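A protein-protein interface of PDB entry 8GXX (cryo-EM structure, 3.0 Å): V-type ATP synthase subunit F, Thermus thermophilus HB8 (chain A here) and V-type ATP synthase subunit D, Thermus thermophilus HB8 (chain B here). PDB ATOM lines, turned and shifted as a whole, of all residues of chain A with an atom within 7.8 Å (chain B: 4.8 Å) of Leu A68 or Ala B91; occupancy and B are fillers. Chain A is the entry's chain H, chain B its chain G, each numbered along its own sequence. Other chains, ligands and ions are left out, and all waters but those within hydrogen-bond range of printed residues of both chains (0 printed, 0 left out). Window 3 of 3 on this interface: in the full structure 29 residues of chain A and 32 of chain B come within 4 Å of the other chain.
Printed residues of chain A within 4 Å of Ala B91: Leu A68.
Printed residues of chain B within 4 Å of Ala A43: Leu B104.
Of the printed residues of chain B, Leu A44 touches Leu B104.
The nearest printed residue of chain B that does not touch Leu A68 is Leu B104 (5.3 Å).
The nearest printed residue of chain B that does not touch Leu A44 is Val B89 (6.4 Å).
O of Ala A43 is in hydrogen-bond range of N of Val A70 (3.2 Å).
Among the printed residues, pairs that only touch across the chains: Met A1 with Val B89 (3.3 Å), Ala A43 with Leu B104 (3.7 Å), Leu A44 with Leu B104 (3.8 Å), Leu A68 with Ala B91 (3.95 Å), Leu A68 with Pro B102 (3.5 Å) and Val A70 with Leu B104 (3.9 Å).
Of the 14 printed residues of chain A, 5 touch a printed residue of chain B.
Printed residues of chain A that touch a printed residue of chain B: Met A1, Ala A43, Leu A44, Leu A68 and Val A70.
Among the printed residues, 6 pairs touch across the chains.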
ATOM      1  N   MET A   1     -11.088 -31.638 -23.766  1.00  0.00           N
ATOM      2  CA  MET A   1     -10.511 -30.625 -22.836  1.00  0.00           C
ATOM      3  C   MET A   1      -9.793 -31.303 -21.676  1.00  0.00           C
ATOM      4  O   MET A   1     -10.137 -32.420 -21.292  1.00  0.00           O
ATOM      5  CB  MET A   1     -11.608 -29.706 -22.301  1.00  0.00           C
ATOM      6  CG  MET A   1     -12.555 -30.376 -21.318  1.00  0.00           C
ATOM      7  SD  MET A   1     -13.977 -29.347 -20.911  1.00  0.00           S
ATOM      8  CE  MET A   1     -14.910 -29.440 -22.436  1.00  0.00           C
ATOM      9  N   GLY A  41      -7.807 -30.340 -30.805  1.00  0.00           N
ATOM     10  CA  GLY A  41      -8.891 -31.100 -30.192  1.00  0.00           C
ATOM     11  C   GLY A  41      -9.360 -30.563 -28.858  1.00  0.00           C
ATOM     12  O   GLY A  41     -10.562 -30.443 -28.625  1.00  0.00           O
ATOM     13  N   TYR A  42      -8.422 -30.238 -27.973  1.00  0.00           N
ATOM     14  CA  TYR A  42      -8.778 -29.718 -26.659  1.00  0.00           C
ATOM     15  C   TYR A  42      -9.418 -28.344 -26.806  1.00  0.00           C
ATOM     16  O   TYR A  42      -8.853 -27.454 -27.449  1.00  0.00           O
ATOM     17  CB  TYR A  42      -7.543 -29.640 -25.766  1.00  0.00           C
ATOM     18  CG  TYR A  42      -6.957 -30.984 -25.384  1.00  0.00           C
ATOM     19  CD1 TYR A  42      -7.465 -32.168 -25.905  1.00  0.00           C
ATOM     20  CD2 TYR A  42      -5.898 -31.068 -24.489  1.00  0.00           C
ATOM     21  CE1 TYR A  42      -6.931 -33.391 -25.552  1.00  0.00           C
ATOM     22  CE2 TYR A  42      -5.359 -32.289 -24.131  1.00  0.00           C
ATOM     23  CZ  TYR A  42      -5.878 -33.446 -24.666  1.00  0.00           C
ATOM     24  OH  TYR A  42      -5.344 -34.664 -24.310  1.00  0.00           O
ATOM     25  N   ALA A  43     -10.599 -28.174 -26.216  1.00  0.00           N
ATOM     26  CA  ALA A  43     -11.327 -26.917 -26.266  1.00  0.00           C
ATOM     27  C   ALA A  43     -11.185 -26.095 -24.993  1.00  0.00           C
ATOM     28  O   ALA A  43     -11.768 -25.010 -24.907  1.00  0.00           O
ATOM     29  CB  ALA A  43     -12.809 -27.179 -26.543  1.00  0.00           C
ATOM     30  N   LEU A  44     -10.436 -26.577 -24.005  1.00  0.00           N
ATOM     31  CA  LEU A  44     -10.252 -25.841 -22.762  1.00  0.00           C
ATOM     32  C   LEU A  44      -9.119 -26.486 -21.984  1.00  0.00           C
ATOM     33  O   LEU A  44      -9.123 -27.702 -21.778  1.00  0.00           O
ATOM     34  CB  LEU A  44     -11.539 -25.835 -21.930  1.00  0.00           C
ATOM     35  CG  LEU A  44     -11.591 -24.848 -20.766  1.00  0.00           C
ATOM     36  CD1 LEU A  44     -13.011 -24.750 -20.236  1.00  0.00           C
ATOM     37  CD2 LEU A  44     -10.636 -25.234 -19.648  1.00  0.00           C
ATOM     38  N   MET A  63      -1.404 -19.481 -29.755  1.00  0.00           N
ATOM     39  CA  MET A  63      -2.842 -19.362 -29.956  1.00  0.00           C
ATOM     40  C   MET A  63      -3.266 -18.048 -30.595  1.00  0.00           C
ATOM     41  O   MET A  63      -4.468 -17.800 -30.725  1.00  0.00           O
ATOM     42  CB  MET A  63      -3.557 -19.541 -28.616  1.00  0.00           C
ATOM     43  CG  MET A  63      -3.132 -20.798 -27.885  1.00  0.00           C
ATOM     44  SD  MET A  63      -3.111 -22.218 -28.988  1.00  0.00           S
ATOM     45  CE  MET A  63      -4.834 -22.303 -29.416  1.00  0.00           C
ATOM     46  N   ARG A  64      -2.321 -17.203 -31.006  1.00  0.00           N
ATOM     47  CA  ARG A  64      -2.712 -15.942 -31.626  1.00  0.00           C
ATOM     48  C   ARG A  64      -3.350 -16.163 -32.991  1.00  0.00           C
ATOM     49  O   ARG A  64      -4.026 -15.265 -33.509  1.00  0.00           O
ATOM     50  CB  ARG A  64      -1.504 -15.014 -31.736  1.00  0.00           C
ATOM     51  CG  ARG A  64      -1.170 -14.311 -30.428  1.00  0.00           C
ATOM     52  CD  ARG A  64       0.106 -13.488 -30.519  1.00  0.00           C
ATOM     53  NE  ARG A  64      -0.002 -12.387 -31.468  1.00  0.00           N
ATOM     54  CZ  ARG A  64       0.891 -11.414 -31.589  1.00  0.00           C
ATOM     55  NH1 ARG A  64       1.968 -11.364 -30.821  1.00  0.00           N
ATOM     56  NH2 ARG A  64       0.698 -10.464 -32.501  1.00  0.00           N
ATOM     57  N   GLY A  65      -3.154 -17.338 -33.586  1.00  0.00           N
ATOM     58  CA  GLY A  65      -3.753 -17.651 -34.869  1.00  0.00           C
ATOM     59  C   GLY A  65      -4.823 -18.722 -34.802  1.00  0.00           C
ATOM     60  O   GLY A  65      -5.605 -18.882 -35.743  1.00  0.00           O
ATOM     61  N   ARG A  66      -4.873 -19.460 -33.696  1.00  0.00           N
ATOM     62  CA  ARG A  66      -5.784 -20.590 -33.523  1.00  0.00           C
ATOM     63  C   ARG A  66      -6.466 -20.516 -32.165  1.00  0.00           C
ATOM     64  O   ARG A  66      -6.586 -21.506 -31.441  1.00  0.00           O
ATOM     65  CB  ARG A  66      -5.031 -21.909 -33.677  1.00  0.00           C
ATOM     66  CG  ARG A  66      -3.740 -21.974 -32.868  1.00  0.00           C
ATOM     67  CD  ARG A  66      -3.099 -23.353 -32.914  1.00  0.00           C
ATOM     68  NE  ARG A  66      -3.873 -24.349 -32.183  1.00  0.00           N
ATOM     69  CZ  ARG A  66      -3.468 -25.591 -31.951  1.00  0.00           C
ATOM     70  NH1 ARG A  66      -2.295 -26.028 -32.383  1.00  0.00           N
ATOM     71  NH2 ARG A  66      -4.256 -26.414 -31.266  1.00  0.00           N
ATOM     72  N   ASP A  67      -6.983 -19.338 -31.827  1.00  0.00           N
ATOM     73  CA  ASP A  67      -7.382 -19.006 -30.466  1.00  0.00           C
ATOM     74  C   ASP A  67      -8.665 -19.705 -30.014  1.00  0.00           C
ATOM     75  O   ASP A  67      -9.277 -19.257 -29.039  1.00  0.00           O
ATOM     76  CB  ASP A  67      -7.552 -17.491 -30.333  1.00  0.00           C
ATOM     77  CG  ASP A  67      -8.586 -16.934 -31.293  1.00  0.00           C
ATOM     78  OD1 ASP A  67      -9.123 -17.715 -32.106  1.00  0.00           O
ATOM     79  OD2 ASP A  67      -8.860 -15.717 -31.234  1.00  0.00           O
ATOM     80  N   LEU A  68      -9.088 -20.769 -30.694  1.00  0.00           N
ATOM     81  CA  LEU A  68     -10.331 -21.454 -30.342  1.00  0.00           C
ATOM     82  C   LEU A  68     -10.410 -21.890 -28.881  1.00  0.00           C
ATOM     83  O   LEU A  68     -11.413 -21.570 -28.225  1.00  0.00           O
ATOM     84  CB  LEU A  68     -10.503 -22.662 -31.272  1.00  0.00           C
ATOM     85  CG  LEU A  68     -11.728 -23.548 -31.028  1.00  0.00           C
ATOM     86  CD1 LEU A  68     -13.018 -22.776 -31.270  1.00  0.00           C
ATOM     87  CD2 LEU A  68     -11.667 -24.786 -31.909  1.00  0.00           C
ATOM     88  N   PRO A  69      -9.432 -22.599 -28.314  1.00  0.00           N
ATOM     89  CA  PRO A  69      -9.604 -23.120 -26.953  1.00  0.00           C
ATOM     90  C   PRO A  69      -9.500 -22.026 -25.906  1.00  0.00           C
ATOM     91  O   PRO A  69      -8.858 -20.994 -26.113  1.00  0.00           O
ATOM     92  CB  PRO A  69      -8.460 -24.129 -26.816  1.00  0.00           C
ATOM     93  CG  PRO A  69      -7.404 -23.573 -27.652  1.00  0.00           C
ATOM     94  CD  PRO A  69      -8.088 -22.909 -28.832  1.00  0.00           C
ATOM     95  N   VAL A  70     -10.143 -22.270 -24.767  1.00  0.00           N
ATOM     96  CA  VAL A  70     -10.228 -21.291 -23.692  1.00  0.00           C
ATOM     97  C   VAL A  70      -9.231 -21.705 -22.618  1.00  0.00           C
ATOM     98  O   VAL A  70      -9.469 -22.645 -21.861  1.00  0.00           O
ATOM     99  CB  VAL A  70     -11.647 -21.186 -23.132  1.00  0.00           C
ATOM    100  CG1 VAL A  70     -11.712 -20.114 -22.054  1.00  0.00           C
ATOM    101  CG2 VAL A  70     -12.641 -20.889 -24.245  1.00  0.00           C
ATOM    102  N   LEU A  71      -8.110 -20.999 -22.555  1.00  0.00           N
ATOM    103  CA  LEU A  71      -7.154 -21.187 -21.476  1.00  0.00           C
ATOM    104  C   LEU A  71      -7.625 -20.398 -20.265  1.00  0.00           C
ATOM    105  O   LEU A  71      -7.970 -19.219 -20.385  1.00  0.00           O
ATOM    106  CB  LEU A  71      -5.764 -20.734 -21.913  1.00  0.00           C
ATOM    107  CG  LEU A  71      -5.363 -21.229 -23.306  1.00  0.00           C
ATOM    108  CD1 LEU A  71      -3.962 -20.767 -23.657  1.00  0.00           C
ATOM    109  CD2 LEU A  71      -5.473 -22.745 -23.398  1.00  0.00           C
ATOM    110  N   VAL B  89     -18.346 -30.785 -24.330  1.00  0.00           N
ATOM    111  CA  VAL B  89     -18.877 -29.555 -24.904  1.00  0.00           C
ATOM    112  C   VAL B  89     -18.641 -29.556 -26.408  1.00  0.00           C
ATOM    113  O   VAL B  89     -17.910 -30.386 -26.953  1.00  0.00           O
ATOM    114  CB  VAL B  89     -18.242 -28.294 -24.278  1.00  0.00           C
ATOM    115  CG1 VAL B  89     -18.276 -28.363 -22.761  1.00  0.00           C
ATOM    116  CG2 VAL B  89     -16.816 -28.106 -24.782  1.00  0.00           C
ATOM    117  N   GLU B  90     -19.280 -28.599 -27.076  1.00  0.00           N
ATOM    118  CA  GLU B  90     -19.020 -28.283 -28.473  1.00  0.00           C
ATOM    119  C   GLU B  90     -18.684 -26.801 -28.554  1.00  0.00           C
ATOM    120  O   GLU B  90     -19.462 -25.962 -28.088  1.00  0.00           O
ATOM    121  CB  GLU B  90     -20.225 -28.619 -29.354  1.00  0.00           C
ATOM    122  CG  GLU B  90     -20.010 -28.347 -30.836  1.00  0.00           C
ATOM    123  CD  GLU B  90     -21.210 -28.732 -31.679  1.00  0.00           C
ATOM    124  OE1 GLU B  90     -22.228 -29.174 -31.103  1.00  0.00           O
ATOM    125  OE2 GLU B  90     -21.138 -28.593 -32.918  1.00  0.00           O
ATOM    126  N   ALA B  91     -17.527 -26.482 -29.135  1.00  0.00           N
ATOM    127  CA  ALA B  91     -17.036 -25.105 -29.185  1.00  0.00           C
ATOM    128  C   ALA B  91     -17.665 -24.381 -30.375  1.00  0.00           C
ATOM    129  O   ALA B  91     -17.021 -24.070 -31.378  1.00  0.00           O
ATOM    130  CB  ALA B  91     -15.516 -25.086 -29.259  1.00  0.00           C
ATOM    131  N   GLU B  92     -18.961 -24.112 -30.246  1.00  0.00           N
ATOM    132  CA  GLU B  92     -19.675 -23.402 -31.294  1.00  0.00           C
ATOM    133  C   GLU B  92     -19.291 -21.928 -31.297  1.00  0.00           C
ATOM    134  O   GLU B  92     -18.888 -21.363 -30.276  1.00  0.00           O
ATOM    135  CB  GLU B  92     -21.184 -23.551 -31.114  1.00  0.00           C
ATOM    136  CG  GLU B  92     -21.717 -23.017 -29.800  1.00  0.00           C
ATOM    137  CD  GLU B  92     -23.226 -23.122 -29.702  1.00  0.00           C
ATOM    138  OE1 GLU B  92     -23.839 -23.745 -30.594  1.00  0.00           O
ATOM    139  OE2 GLU B  92     -23.800 -22.582 -28.734  1.00  0.00           O
ATOM    140  N   VAL B  93     -19.423 -21.303 -32.463  1.00  0.00           N
ATOM    141  CA  VAL B  93     -19.068 -19.900 -32.639  1.00  0.00           C
ATOM    142  C   VAL B  93     -20.249 -19.032 -32.230  1.00  0.00           C
ATOM    143  O   VAL B  93     -21.374 -19.229 -32.702  1.00  0.00           O
ATOM    144  CB  VAL B  93     -18.646 -19.613 -34.091  1.00  0.00           C
ATOM    145  CG1 VAL B  93     -17.384 -20.389 -34.438  1.00  0.00           C
ATOM    146  CG2 VAL B  93     -19.770 -19.950 -35.071  1.00  0.00           C
ATOM    147  N   PRO B 102     -15.953 -18.211 -29.119  1.00  0.00           N
ATOM    148  CA  PRO B 102     -16.481 -19.574 -29.009  1.00  0.00           C
ATOM    149  C   PRO B 102     -17.309 -19.753 -27.750  1.00  0.00           C
ATOM    150  O   PRO B 102     -16.926 -19.316 -26.662  1.00  0.00           O
ATOM    151  CB  PRO B 102     -15.212 -20.432 -28.964  1.00  0.00           C
ATOM    152  CG  PRO B 102     -14.213 -19.554 -28.293  1.00  0.00           C
ATOM    153  CD  PRO B 102     -14.545 -18.135 -28.687  1.00  0.00           C
ATOM    154  N   ARG B 103     -18.455 -20.407 -27.905  1.00  0.00           N
ATOM    155  CA  ARG B 103     -19.290 -20.813 -26.781  1.00  0.00           C
ATOM    156  C   ARG B 103     -19.177 -22.324 -26.632  1.00  0.00           C
ATOM    157  O   ARG B 103     -19.632 -23.077 -27.500  1.00  0.00           O
ATOM    158  CB  ARG B 103     -20.740 -20.388 -26.981  1.00  0.00           C
ATOM    159  CG  ARG B 103     -21.047 -19.019 -26.409  1.00  0.00           C
ATOM    160  CD  ARG B 103     -22.519 -18.671 -26.543  1.00  0.00           C
ATOM    161  NE  ARG B 103     -23.375 -19.568 -25.777  1.00  0.00           N
ATOM    162  CZ  ARG B 103     -24.696 -19.475 -25.720  1.00  0.00           C
ATOM    163  NH1 ARG B 103     -25.352 -18.533 -26.378  1.00  0.00           N
ATOM    164  NH2 ARG B 103     -25.377 -20.347 -24.982  1.00  0.00           N
ATOM    165  N   LEU B 104     -18.571 -22.763 -25.531  1.00  0.00           N
ATOM    166  CA  LEU B 104     -18.388 -24.184 -25.254  1.00  0.00           C
ATOM    167  C   LEU B 104     -19.725 -24.760 -24.793  1.00  0.00           C
ATOM    168  O   LEU B 104     -19.948 -25.045 -23.614  1.00  0.00           O
ATOM    169  CB  LEU B 104     -17.300 -24.385 -24.211  1.00  0.00           C
ATOM    170  CG  LEU B 104     -15.958 -23.716 -24.512  1.00  0.00           C
ATOM    171  CD1 LEU B 104     -14.987 -23.937 -23.363  1.00  0.00           C
ATOM    172  CD2 LEU B 104     -15.374 -24.231 -25.817  1.00  0.00           C
